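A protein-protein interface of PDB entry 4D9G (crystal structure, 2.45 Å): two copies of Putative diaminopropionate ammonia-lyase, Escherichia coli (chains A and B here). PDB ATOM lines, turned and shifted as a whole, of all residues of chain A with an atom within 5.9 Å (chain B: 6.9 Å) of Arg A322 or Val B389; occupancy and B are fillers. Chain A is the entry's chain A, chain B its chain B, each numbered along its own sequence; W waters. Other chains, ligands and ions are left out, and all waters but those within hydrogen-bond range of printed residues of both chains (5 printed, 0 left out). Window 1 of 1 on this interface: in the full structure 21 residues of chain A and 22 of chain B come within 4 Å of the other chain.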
ATOM      1  N   SER A 315     -30.676  19.219  -5.562  1.00  0.00           N
ATOM      2  CA  SER A 315     -30.233  19.952  -6.727  1.00  0.00           C
ATOM      3  C   SER A 315     -28.725  19.887  -6.915  1.00  0.00           C
ATOM      4  O   SER A 315     -28.198  20.336  -7.923  1.00  0.00           O
ATOM      5  CB  SER A 315     -30.715  21.398  -6.635  1.00  0.00           C
ATOM      6  OG  SER A 315     -30.295  21.969  -5.426  1.00  0.00           O
ATOM      7  N   ALA A 317     -27.108  17.166  -7.361  1.00  0.00           N
ATOM      8  CA  ALA A 317     -26.945  16.196  -8.438  1.00  0.00           C
ATOM      9  C   ALA A 317     -27.171  16.833  -9.823  1.00  0.00           C
ATOM     10  O   ALA A 317     -26.380  16.619 -10.747  1.00  0.00           O
ATOM     11  CB  ALA A 317     -27.872  15.003  -8.223  1.00  0.00           C
ATOM     12  N   ALA A 318     -28.246  17.606  -9.961  1.00  0.00           N
ATOM     13  CA  ALA A 318     -28.492  18.364 -11.186  1.00  0.00           C
ATOM     14  C   ALA A 318     -27.311  19.285 -11.550  1.00  0.00           C
ATOM     15  O   ALA A 318     -26.957  19.401 -12.725  1.00  0.00           O
ATOM     16  CB  ALA A 318     -29.784  19.154 -11.073  1.00  0.00           C
ATOM     17  N   LEU A 319     -26.696  19.915 -10.545  1.00  0.00           N
ATOM     18  CA  LEU A 319     -25.472  20.705 -10.742  1.00  0.00           C
ATOM     19  C   LEU A 319     -24.367  19.842 -11.356  1.00  0.00           C
ATOM     20  O   LEU A 319     -23.809  20.188 -12.405  1.00  0.00           O
ATOM     21  CB  LEU A 319     -25.002  21.341  -9.420  1.00  0.00           C
ATOM     22  CG  LEU A 319     -23.697  22.175  -9.342  1.00  0.00           C
ATOM     23  CD1 LEU A 319     -23.697  23.370 -10.289  1.00  0.00           C
ATOM     24  CD2 LEU A 319     -23.416  22.633  -7.917  1.00  0.00           C
ATOM     25  N   GLY A 320     -24.077  18.710 -10.707  1.00  0.00           N
ATOM     26  CA  GLY A 320     -23.061  17.767 -11.189  1.00  0.00           C
ATOM     27  C   GLY A 320     -23.272  17.325 -12.634  1.00  0.00           C
ATOM     28  O   GLY A 320     -22.316  17.202 -13.401  1.00  0.00           O
ATOM     29  N   MET A 321     -24.527  17.089 -13.009  1.00  0.00           N
ATOM     30  CA  MET A 321     -24.858  16.670 -14.367  1.00  0.00           C
ATOM     31  C   MET A 321     -24.395  17.704 -15.362  1.00  0.00           C
ATOM     32  O   MET A 321     -23.740  17.372 -16.356  1.00  0.00           O
ATOM     33  CB  MET A 321     -26.367  16.462 -14.500  1.00  0.00           C
ATOM     34  CG  MET A 321     -26.841  15.232 -13.760  1.00  0.00           C
ATOM     35  SD  MET A 321     -28.805  15.216 -13.618  1.00  0.00           S
ATOM     36  CE  MET A 321     -29.227  14.669 -15.467  1.00  0.00           C
ATOM     37  N   ARG A 322     -24.732  18.965 -15.091  1.00  0.00           N
ATOM     38  CA  ARG A 322     -24.437  20.071 -15.995  1.00  0.00           C
ATOM     39  C   ARG A 322     -22.940  20.383 -16.040  1.00  0.00           C
ATOM     40  O   ARG A 322     -22.409  20.738 -17.091  1.00  0.00           O
ATOM     41  CB  ARG A 322     -25.210  21.312 -15.579  1.00  0.00           C
ATOM     42  CG  ARG A 322     -26.712  21.196 -15.704  1.00  0.00           C
ATOM     43  CD  ARG A 322     -27.371  22.516 -15.344  1.00  0.00           C
ATOM     44  NE  ARG A 322     -28.766  22.348 -14.953  1.00  0.00           N
ATOM     45  CZ  ARG A 322     -29.215  22.467 -13.713  1.00  0.00           C
ATOM     46  NH1 ARG A 322     -28.401  22.795 -12.724  1.00  0.00           N
ATOM     47  NH2 ARG A 322     -30.489  22.273 -13.474  1.00  0.00           N
ATOM     48  N   VAL A 323     -22.273  20.262 -14.899  1.00  0.00           N
ATOM     49  CA  VAL A 323     -20.840  20.515 -14.820  1.00  0.00           C
ATOM     50  C   VAL A 323     -20.090  19.440 -15.613  1.00  0.00           C
ATOM     51  O   VAL A 323     -19.117  19.740 -16.311  1.00  0.00           O
ATOM     52  CB  VAL A 323     -20.317  20.566 -13.351  1.00  0.00           C
ATOM     53  CG1 VAL A 323     -18.799  20.671 -13.328  1.00  0.00           C
ATOM     54  CG2 VAL A 323     -20.943  21.742 -12.588  1.00  0.00           C
ATOM     55  N   LEU A 324     -20.557  18.203 -15.516  1.00  0.00           N
ATOM     56  CA  LEU A 324     -19.935  17.104 -16.253  1.00  0.00           C
ATOM     57  C   LEU A 324     -20.185  17.198 -17.751  1.00  0.00           C
ATOM     58  O   LEU A 324     -19.288  16.943 -18.550  1.00  0.00           O
ATOM     59  CB  LEU A 324     -20.364  15.737 -15.694  1.00  0.00           C
ATOM     60  CG  LEU A 324     -19.629  15.381 -14.388  1.00  0.00           C
ATOM     61  CD1 LEU A 324     -20.300  14.231 -13.654  1.00  0.00           C
ATOM     62  CD2 LEU A 324     -18.147  15.087 -14.627  1.00  0.00           C
ATOM     63  N   GLY A 325     -21.414  17.573 -18.104  1.00  0.00           N
ATOM     64  CA  GLY A 325     -21.848  17.636 -19.486  1.00  0.00           C
ATOM     65  C   GLY A 325     -21.330  18.826 -20.271  1.00  0.00           C
ATOM     66  O   GLY A 325     -21.226  18.756 -21.491  1.00  0.00           O
ATOM     67  N   ASN A 326     -21.029  19.917 -19.569  1.00  0.00           N
ATOM     68  CA  ASN A 326     -20.448  21.100 -20.181  1.00  0.00           C
ATOM     69  C   ASN A 326     -19.197  21.508 -19.399  1.00  0.00           C
ATOM     70  O   ASN A 326     -19.250  22.420 -18.571  1.00  0.00           O
ATOM     71  CB  ASN A 326     -21.466  22.238 -20.214  1.00  0.00           C
ATOM     72  CG  ASN A 326     -21.047  23.368 -21.121  1.00  0.00           C
ATOM     73  OD1 ASN A 326     -19.870  23.527 -21.428  1.00  0.00           O
ATOM     74  ND2 ASN A 326     -22.017  24.175 -21.551  1.00  0.00           N
ATOM     75  N   PRO A 327     -18.065  20.828 -19.665  1.00  0.00           N
ATOM     76  CA  PRO A 327     -16.846  20.983 -18.856  1.00  0.00           C
ATOM     77  C   PRO A 327     -16.227  22.392 -18.878  1.00  0.00           C
ATOM     78  O   PRO A 327     -16.573  23.214 -19.726  1.00  0.00           O
ATOM     79  CB  PRO A 327     -15.883  19.939 -19.459  1.00  0.00           C
ATOM     80  CG  PRO A 327     -16.394  19.701 -20.838  1.00  0.00           C
ATOM     81  CD  PRO A 327     -17.882  19.864 -20.769  1.00  0.00           C
ATOM     82  N   GLU A 387     -33.736  17.682 -19.962  1.00  0.00           N
ATOM     83  CA  GLU A 387     -34.487  18.664 -19.168  1.00  0.00           C
ATOM     84  C   GLU A 387     -33.580  19.385 -18.174  1.00  0.00           C
ATOM     85  O   GLU A 387     -33.637  20.608 -18.057  1.00  0.00           O
ATOM     86  CB  GLU A 387     -35.674  18.031 -18.444  1.00  0.00           C
ATOM     87  CG  GLU A 387     -36.863  17.750 -19.347  1.00  0.00           C
ATOM     88  CD  GLU A 387     -37.872  16.803 -18.722  1.00  0.00           C
ATOM     89  OE1 GLU A 387     -37.571  16.189 -17.671  1.00  0.00           O
ATOM     90  OE2 GLU A 387     -38.980  16.669 -19.287  1.00  0.00           O
ATOM     91  N   VAL A 388     -32.731  18.624 -17.485  1.00  0.00           N
ATOM     92  CA  VAL A 388     -31.733  19.197 -16.583  1.00  0.00           C
ATOM     93  C   VAL A 388     -30.670  20.038 -17.325  1.00  0.00           C
ATOM     94  O   VAL A 388     -30.438  21.205 -16.969  1.00  0.00           O
ATOM     95  CB  VAL A 388     -31.050  18.100 -15.728  1.00  0.00           C
ATOM     96  CG1 VAL A 388     -29.870  18.679 -14.944  1.00  0.00           C
ATOM     97  CG2 VAL A 388     -32.067  17.423 -14.807  1.00  0.00           C
ATOM     98  N   VAL A 389     -30.043  19.462 -18.354  1.00  0.00           N
ATOM     99  CA  VAL A 389     -28.910  20.135 -19.014  1.00  0.00           C
ATOM    100  C   VAL A 389     -29.279  21.217 -20.017  1.00  0.00           C
ATOM    101  O   VAL A 389     -28.526  22.164 -20.197  1.00  0.00           O
ATOM    102  CB  VAL A 389     -27.871  19.157 -19.629  1.00  0.00           C
ATOM    103  CG1 VAL A 389     -27.369  18.170 -18.570  1.00  0.00           C
ATOM    104  CG2 VAL A 389     -28.412  18.458 -20.883  1.00  0.00           C
ATOM    105  N   GLY A 392     -32.778  23.606 -17.911  1.00  0.00           N
ATOM    106  CA  GLY A 392     -32.447  24.179 -16.617  1.00  0.00           C
ATOM    107  C   GLY A 392     -33.338  23.702 -15.483  1.00  0.00           C
ATOM    108  O   GLY A 392     -33.415  24.347 -14.430  1.00  0.00           O
ATOM    109  N   LYS A 393     -34.022  22.579 -15.700  1.00  0.00           N
ATOM    110  CA  LYS A 393     -34.832  21.939 -14.658  1.00  0.00           C
ATOM    111  C   LYS A 393     -33.961  21.589 -13.454  1.00  0.00           C
ATOM    112  O   LYS A 393     -32.819  21.167 -13.618  1.00  0.00           O
ATOM    113  CB  LYS A 393     -35.532  20.693 -15.224  1.00  0.00           C
ATOM    114  CG  LYS A 393     -36.030  19.677 -14.196  1.00  0.00           C
ATOM    115  CD  LYS A 393     -36.828  18.577 -14.883  1.00  0.00           C
ATOM    116  CE  LYS A 393     -36.552  17.220 -14.254  1.00  0.00           C
ATOM    117  NZ  LYS A 393     -37.192  16.100 -15.004  1.00  0.00           N
ATOM    118  N   HIS A 394     -34.525  21.760 -12.258  1.00  0.00           N
ATOM    119  CA  HIS A 394     -33.806  21.637 -10.977  1.00  0.00           C
ATOM    120  C   HIS A 394     -32.661  22.619 -10.870  1.00  0.00           C
ATOM    121  O   HIS A 394     -31.539  22.255 -10.482  1.00  0.00           O
ATOM    122  CB  HIS A 394     -33.361  20.196 -10.695  1.00  0.00           C
ATOM    123  CG  HIS A 394     -34.502  19.208 -10.641  1.00  0.00           C
ATOM    124  ND1 HIS A 394     -34.429  17.976 -11.198  1.00  0.00           N
ATOM    125  CD2 HIS A 394     -35.780  19.310 -10.087  1.00  0.00           C
ATOM    126  CE1 HIS A 394     -35.589  17.322 -10.998  1.00  0.00           C
ATOM    127  NE2 HIS A 394     -36.420  18.142 -10.328  1.00  0.00           N
ATOM    128  N   ALA A 395     -32.953  23.880 -11.202  1.00  0.00           N
ATOM    129  CA  ALA A 395     -31.990  24.969 -11.113  1.00  0.00           C
ATOM    130  C   ALA A 395     -31.481  25.175  -9.689  1.00  0.00           C
ATOM    131  O   ALA A 395     -32.128  24.785  -8.711  1.00  0.00           O
ATOM    132  CB  ALA A 395     -32.603  26.255 -11.646  1.00  0.00           C
ATOM    133  N   VAL A 396     -30.312  25.793  -9.589  1.00  0.00           N
ATOM    134  CA  VAL A 396     -29.659  26.068  -8.315  1.00  0.00           C
ATOM    135  C   VAL A 396     -30.455  27.038  -7.417  1.00  0.00           C
ATOM    136  O   VAL A 396     -30.561  26.821  -6.203  1.00  0.00           O
ATOM    137  CB  VAL A 396     -28.228  26.580  -8.562  1.00  0.00           C
ATOM    138  CG1 VAL A 396     -27.729  27.432  -7.405  1.00  0.00           C
ATOM    139  CG2 VAL A 396     -27.292  25.418  -8.830  1.00  0.00           C
ATOM    140  N   ALA B 318     -30.847  31.537 -23.600  1.00  0.00           N
ATOM    141  CA  ALA B 318     -30.258  30.689 -22.571  1.00  0.00           C
ATOM    142  C   ALA B 318     -30.366  29.207 -22.948  1.00  0.00           C
ATOM    143  O   ALA B 318     -29.429  28.428 -22.728  1.00  0.00           O
ATOM    144  CB  ALA B 318     -30.921  30.948 -21.222  1.00  0.00           C
ATOM    145  N   MET B 321     -27.700  28.459 -25.495  1.00  0.00           N
ATOM    146  CA  MET B 321     -26.372  28.372 -24.892  1.00  0.00           C
ATOM    147  C   MET B 321     -26.122  26.969 -24.397  1.00  0.00           C
ATOM    148  O   MET B 321     -25.024  26.421 -24.558  1.00  0.00           O
ATOM    149  CB  MET B 321     -26.278  29.326 -23.707  1.00  0.00           C
ATOM    150  CG  MET B 321     -26.254  30.779 -24.144  1.00  0.00           C
ATOM    151  SD  MET B 321     -26.464  31.954 -22.582  1.00  0.00           S
ATOM    152  CE  MET B 321     -24.696  31.742 -21.741  1.00  0.00           C
ATOM    153  N   ARG B 322     -27.159  26.384 -23.796  1.00  0.00           N
ATOM    154  CA  ARG B 322     -27.067  25.088 -23.155  1.00  0.00           C
ATOM    155  C   ARG B 322     -27.036  23.974 -24.186  1.00  0.00           C
ATOM    156  O   ARG B 322     -26.235  23.043 -24.059  1.00  0.00           O
ATOM    157  CB  ARG B 322     -28.219  24.888 -22.156  1.00  0.00           C
ATOM    158  CG  ARG B 322     -28.170  25.819 -20.954  1.00  0.00           C
ATOM    159  CD  ARG B 322     -29.209  25.414 -19.922  1.00  0.00           C
ATOM    160  NE  ARG B 322     -29.643  26.550 -19.111  1.00  0.00           N
ATOM    161  CZ  ARG B 322     -30.757  27.245 -19.313  1.00  0.00           C
ATOM    162  NH1 ARG B 322     -31.584  26.932 -20.286  1.00  0.00           N
ATOM    163  NH2 ARG B 322     -31.039  28.259 -18.531  1.00  0.00           N
ATOM    164  N   VAL B 323     -27.903  24.089 -25.196  1.00  0.00           N
ATOM    165  CA  VAL B 323     -28.014  23.110 -26.271  1.00  0.00           C
ATOM    166  C   VAL B 323     -26.684  22.988 -27.042  1.00  0.00           C
ATOM    167  O   VAL B 323     -26.246  21.881 -27.371  1.00  0.00           O
ATOM    168  CB  VAL B 323     -29.221  23.433 -27.208  1.00  0.00           C
ATOM    169  CG1 VAL B 323     -29.283  22.480 -28.401  1.00  0.00           C
ATOM    170  CG2 VAL B 323     -30.541  23.370 -26.430  1.00  0.00           C
ATOM    171  N   GLY B 325     -23.726  23.992 -25.772  1.00  0.00           N
ATOM    172  CA  GLY B 325     -22.686  23.701 -24.806  1.00  0.00           C
ATOM    173  C   GLY B 325     -22.641  22.264 -24.364  1.00  0.00           C
ATOM    174  O   GLY B 325     -21.617  21.804 -23.879  1.00  0.00           O
ATOM    175  N   ASN B 326     -23.756  21.558 -24.529  1.00  0.00           N
ATOM    176  CA  ASN B 326     -23.865  20.145 -24.183  1.00  0.00           C
ATOM    177  C   ASN B 326     -24.679  19.468 -25.291  1.00  0.00           C
ATOM    178  O   ASN B 326     -25.894  19.274 -25.171  1.00  0.00           O
ATOM    179  CB  ASN B 326     -24.481  19.962 -22.792  1.00  0.00           C
ATOM    180  CG  ASN B 326     -24.484  18.506 -22.331  1.00  0.00           C
ATOM    181  OD1 ASN B 326     -24.250  17.581 -23.120  1.00  0.00           O
ATOM    182  ND2 ASN B 326     -24.758  18.296 -21.034  1.00  0.00           N
ATOM    183  N   SER B 336     -21.045  29.182 -26.616  1.00  0.00           N
ATOM    184  CA  SER B 336     -21.807  30.251 -27.196  1.00  0.00           C
ATOM    185  C   SER B 336     -22.440  31.123 -26.126  1.00  0.00           C
ATOM    186  O   SER B 336     -23.241  30.629 -25.323  1.00  0.00           O
ATOM    187  CB  SER B 336     -22.888  29.664 -28.095  1.00  0.00           C
ATOM    188  OG  SER B 336     -23.455  30.658 -28.934  1.00  0.00           O
ATOM    189  N   HIS B 384     -21.546  34.800 -16.308  1.00  0.00           N
ATOM    190  CA  HIS B 384     -22.887  34.626 -16.862  1.00  0.00           C
ATOM    191  C   HIS B 384     -23.031  33.312 -17.594  1.00  0.00           C
ATOM    192  O   HIS B 384     -24.064  32.633 -17.487  1.00  0.00           O
ATOM    193  CB  HIS B 384     -23.254  35.796 -17.764  1.00  0.00           C
ATOM    194  CG  HIS B 384     -24.602  35.656 -18.427  1.00  0.00           C
ATOM    195  ND1 HIS B 384     -25.766  35.867 -17.765  1.00  0.00           N
ATOM    196  CD2 HIS B 384     -24.947  35.309 -19.725  1.00  0.00           C
ATOM    197  CE1 HIS B 384     -26.802  35.662 -18.603  1.00  0.00           C
ATOM    198  NE2 HIS B 384     -26.305  35.322 -19.801  1.00  0.00           N
ATOM    199  N   TYR B 385     -21.987  32.931 -18.329  1.00  0.00           N
ATOM    200  CA  TYR B 385     -22.007  31.668 -19.063  1.00  0.00           C
ATOM    201  C   TYR B 385     -22.264  30.469 -18.136  1.00  0.00           C
ATOM    202  O   TYR B 385     -23.152  29.649 -18.395  1.00  0.00           O
ATOM    203  CB  TYR B 385     -20.710  31.461 -19.868  1.00  0.00           C
ATOM    204  CG  TYR B 385     -20.761  30.228 -20.739  1.00  0.00           C
ATOM    205  CD1 TYR B 385     -21.499  30.231 -21.924  1.00  0.00           C
ATOM    206  CD2 TYR B 385     -20.109  29.048 -20.366  1.00  0.00           C
ATOM    207  CE1 TYR B 385     -21.576  29.109 -22.722  1.00  0.00           C
ATOM    208  CE2 TYR B 385     -20.174  27.912 -21.169  1.00  0.00           C
ATOM    209  CZ  TYR B 385     -20.911  27.954 -22.350  1.00  0.00           C
ATOM    210  OH  TYR B 385     -21.018  26.860 -23.178  1.00  0.00           O
ATOM    211  N   ARG B 386     -21.484  30.379 -17.059  1.00  0.00           N
ATOM    212  CA  ARG B 386     -21.559  29.227 -16.179  1.00  0.00           C
ATOM    213  C   ARG B 386     -22.812  29.250 -15.313  1.00  0.00           C
ATOM    214  O   ARG B 386     -23.323  28.188 -14.938  1.00  0.00           O
ATOM    215  CB  ARG B 386     -20.290  29.067 -15.341  1.00  0.00           C
ATOM    216  CG  ARG B 386     -19.037  28.737 -16.151  1.00  0.00           C
ATOM    217  CD  ARG B 386     -19.172  27.452 -16.959  1.00  0.00           C
ATOM    218  NE  ARG B 386     -18.104  27.338 -17.957  1.00  0.00           N
ATOM    219  CZ  ARG B 386     -17.914  26.292 -18.762  1.00  0.00           C
ATOM    220  NH1 ARG B 386     -18.728  25.237 -18.707  1.00  0.00           N
ATOM    221  NH2 ARG B 386     -16.902  26.304 -19.631  1.00  0.00           N
ATOM    222  N   GLU B 387     -23.318  30.446 -15.017  1.00  0.00           N
ATOM    223  CA  GLU B 387     -24.591  30.573 -14.311  1.00  0.00           C
ATOM    224  C   GLU B 387     -25.712  29.931 -15.133  1.00  0.00           C
ATOM    225  O   GLU B 387     -26.577  29.250 -14.584  1.00  0.00           O
ATOM    226  CB  GLU B 387     -24.910  32.043 -13.994  1.00  0.00           C
ATOM    227  CG  GLU B 387     -24.170  32.584 -12.771  1.00  0.00           C
ATOM    228  CD  GLU B 387     -24.394  34.067 -12.507  1.00  0.00           C
ATOM    229  OE1 GLU B 387     -24.644  34.845 -13.454  1.00  0.00           O
ATOM    230  OE2 GLU B 387     -24.306  34.474 -11.333  1.00  0.00           O
ATOM    231  N   VAL B 388     -25.678  30.141 -16.450  1.00  0.00           N
ATOM    232  CA  VAL B 388     -26.660  29.580 -17.368  1.00  0.00           C
ATOM    233  C   VAL B 388     -26.487  28.067 -17.537  1.00  0.00           C
ATOM    234  O   VAL B 388     -27.442  27.309 -17.335  1.00  0.00           O
ATOM    235  CB  VAL B 388     -26.608  30.296 -18.748  1.00  0.00           C
ATOM    236  CG1 VAL B 388     -27.284  29.467 -19.835  1.00  0.00           C
ATOM    237  CG2 VAL B 388     -27.245  31.686 -18.657  1.00  0.00           C
ATOM    238  N   VAL B 389     -25.277  27.632 -17.891  1.00  0.00           N
ATOM    239  CA  VAL B 389     -25.054  26.237 -18.270  1.00  0.00           C
ATOM    240  C   VAL B 389     -24.864  25.296 -17.080  1.00  0.00           C
ATOM    241  O   VAL B 389     -25.185  24.097 -17.194  1.00  0.00           O
ATOM    242  CB  VAL B 389     -23.930  26.040 -19.321  1.00  0.00           C
ATOM    243  CG1 VAL B 389     -24.191  26.902 -20.557  1.00  0.00           C
ATOM    244  CG2 VAL B 389     -22.537  26.295 -18.743  1.00  0.00           C
ATOM    245  N   TRP B 390     -24.362  25.825 -15.956  1.00  0.00           N
ATOM    246  CA  TRP B 390     -24.148  25.008 -14.756  1.00  0.00           C
ATOM    247  C   TRP B 390     -25.204  25.198 -13.719  1.00  0.00           C
ATOM    248  O   TRP B 390     -25.691  24.228 -13.158  1.00  0.00           O
ATOM    249  CB  TRP B 390     -22.791  25.278 -14.116  1.00  0.00           C
ATOM    250  CG  TRP B 390     -21.612  24.723 -14.870  1.00  0.00           C
ATOM    251  CD1 TRP B 390     -21.626  23.944 -16.017  1.00  0.00           C
ATOM    252  CD2 TRP B 390     -20.200  24.868 -14.520  1.00  0.00           C
ATOM    253  NE1 TRP B 390     -20.353  23.620 -16.399  1.00  0.00           N
ATOM    254  CE2 TRP B 390     -19.447  24.149 -15.544  1.00  0.00           C
ATOM    255  CE3 TRP B 390     -19.506  25.509 -13.492  1.00  0.00           C
ATOM    256  CZ2 TRP B 390     -18.055  24.078 -15.526  1.00  0.00           C
ATOM    257  CZ3 TRP B 390     -18.103  25.426 -13.476  1.00  0.00           C
ATOM    258  CH2 TRP B 390     -17.397  24.732 -14.474  1.00  0.00           C
ATOM    259  N   GLU B 391     -25.556  26.447 -13.435  1.00  0.00           N
ATOM    260  CA  GLU B 391     -26.508  26.732 -12.368  1.00  0.00           C
ATOM    261  C   GLU B 391     -27.950  26.659 -12.856  1.00  0.00           C
ATOM    262  O   GLU B 391     -28.876  26.546 -12.062  1.00  0.00           O
ATOM    263  CB  GLU B 391     -26.226  28.093 -11.725  1.00  0.00           C
ATOM    264  CG  GLU B 391     -24.894  28.177 -11.018  1.00  0.00           C
ATOM    265  CD  GLU B 391     -24.586  29.571 -10.489  1.00  0.00           C
ATOM    266  OE1 GLU B 391     -25.510  30.284 -10.038  1.00  0.00           O
ATOM    267  OE2 GLU B 391     -23.399  29.949 -10.511  1.00  0.00           O
ATOM    268  N   GLY B 392     -28.139  26.732 -14.161  1.00  0.00           N
ATOM    269  CA  GLY B 392     -29.481  26.722 -14.721  1.00  0.00           C
ATOM    270  C   GLY B 392     -30.210  28.051 -14.610  1.00  0.00           C
ATOM    271  O   GLY B 392     -31.430  28.096 -14.727  1.00  0.00           O
ATOM    272  N   LYS B 393     -29.457  29.130 -14.396  1.00  0.00           N
ATOM    273  CA  LYS B 393     -29.998  30.489 -14.403  1.00  0.00           C
ATOM    274  C   LYS B 393     -30.712  30.745 -15.733  1.00  0.00           C
ATOM    275  O   LYS B 393     -30.301  30.217 -16.774  1.00  0.00           O
ATOM    276  CB  LYS B 393     -28.868  31.498 -14.196  1.00  0.00           C
ATOM    277  CG  LYS B 393     -29.288  32.949 -14.020  1.00  0.00           C
ATOM    278  CD  LYS B 393     -28.328  33.862 -14.784  1.00  0.00           C
ATOM    279  CE  LYS B 393     -28.090  35.174 -14.040  1.00  0.00           C
ATOM    280  NZ  LYS B 393     -26.943  35.949 -14.610  1.00  0.00           N
HETATM  281  O   HOH W   1     -24.247  20.400 -19.273  1.00  0.00           O
HETATM  282  O   HOH W   2     -29.997  29.046 -10.824  1.00  0.00           O
HETATM  283  O   HOH W   3     -25.978  22.609 -19.414  1.00  0.00           O
HETATM  284  O   HOH W   4     -15.170  25.117 -21.885  1.00  0.00           O
HETATM  285  O   HOH W   5     -24.670  23.302 -21.707  1.00  0.00           O
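O of Asn A326 is in hydrogen-bond range of NE1 of Trp B390.
The guanidinium group (NH1) of Arg A322 lies within hydrogen-bond range of the backbone carbonyl oxygen (O) of Trp B390.
ND2 of Asn A326 sits close to O of Gly B325 (3.3 Å).
The backbone NH of Val A396 lies within hydrogen-bond range of the backbone carbonyl oxygen of Glu B391.
O of Asn A326 is in hydrogen-bond range of NH1 of Arg B386 (2.9 Å).
The backbone carbonyl oxygen (O) of Pro A327 sits at hydrogen-bond distance from the guanidinium group (NH2) of Arg B386 (3.1 Å).
The side-chain hydroxyl (OH) of Tyr B385 is in hydrogen-bond range of the side-chain amide nitrogen (ND2) of Asn A326 (3.3 Å).
O of His A394 is in hydrogen-bond range of NH2 of Arg A322, at 3.2 Å.
The backbone carbonyl oxygen of Lys B393 lies within hydrogen-bond range of the guanidinium group of Arg B322, 2.7 Å away.
The guanidinium group (NH2) of Arg A322 is in hydrogen-bond range of the backbone carbonyl oxygen (O) of Lys A393 (2.6 Å).
The backbone carbonyl oxygen of Arg B386 is in hydrogen-bond range of the backbone NH of Glu B391 (3.2 Å).
The guanidinium group (NE) of Arg B322 sits at hydrogen-bond distance from the backbone carbonyl oxygen (O) of Val B388 (2.9 Å).
The backbone carbonyl oxygen (O) of Glu B387 sits at hydrogen-bond distance from the backbone NH (N) of Gly B392 (3.0 Å).
Among the printed residues, pairs that only touch across the chains: Leu A319 with Trp B390, Arg A322 with Val B389, Arg A322 with Glu B391, Val A323 with Trp B390, Gly A325 with Gly B325, Gly A325 with Asn B326, Asn A326 with Val B389, Val A389 with Arg B322, Val A389 with Asn B326, Ala A395 with Glu B391 and Ala A395 with Gly B392.
Of the printed residues of chain B, Arg A322 touches Val B389 (3.2 Å), Trp B390 (3.1 Å) and Glu B391 (3.8 Å).
Of chain A, only Arg A322 (3.2 Å) and Asn A326 (3.5 Å) come within 4 Å of Val B389.
Of the printed residues of chain B, Val A396 touches Glu B391 (3.0 Å).
Of the printed residues of chain A, Gly B392 touches Ala A395.
Of the printed residues of chain A, Glu B391 touches Arg A322 (3.8 Å), Ala A395 (3.6 Å) and Val A396 (3.0 Å).
The nearest residue of chain B that does not touch Arg A322 is Gly B392 (4.2 Å).
The nearest residue of chain A that does not touch Val B389 is Val A389 (4.9 Å).
The nearest printed residue of chain B that does not touch Leu A319 is Glu B391 (4.8 Å).
Of the 17 printed residues of chain B, 9 touch a printed residue of chain A.
Along chain B the printed residues that touch a printed residue of chain A span positions 322 to 392.
Of the 20 printed residues of chain A, 9 touch a printed residue of chain B.
Printed residues of chain A that touch a printed residue of chain B: Leu A319, Arg A322, Val A323, Gly A325, Asn A326, Pro A327, Val A389, Ala A395 and Val A396.
Among the printed residues, 18 pairs touch across the chains.
Among the printed residues, no Asp or Glu carboxylate lies within 4 Å of a Lys or Arg side-chain nitrogen of the other chain.
Arg A322 touches Val B389, and with the chains exchanged Val A389 touches Arg B322.
Gly B325 touches its own counterpart, Gly A325.
Gly A325 touches Asn B326, and with the chains exchanged Asn A326 touches Gly B325.
Asn A326 touches Val B389, and with the chains exchanged Val A389 touches Asn B326.
Of the 18 pairs that touch across the chains among the printed residues, 7 have their exchanged pair printed and touching as well.
Water W3 bridges the backbone carbonyl oxygen of Val A389 (2.7 Å) and the backbone carbonyl oxygen of Val B389 (2.8 Å).
Water W1 lies within hydrogen-bond range of ND2 of Asn B326, O of Arg A322 and N of Asn A326.
Water W5 lies within hydrogen-bond range of the side-chain amide nitrogen (ND2) of Asn A326, the backbone carbonyl oxygen (O) of Arg B322 and the backbone NH (N) of Asn B326.
Water W2 lies within hydrogen-bond range of the backbone carbonyl oxygen of Glu B391 and the backbone NH of Val A396.
Water W4 bridges NH2 of Arg B386 and O of Pro A327.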
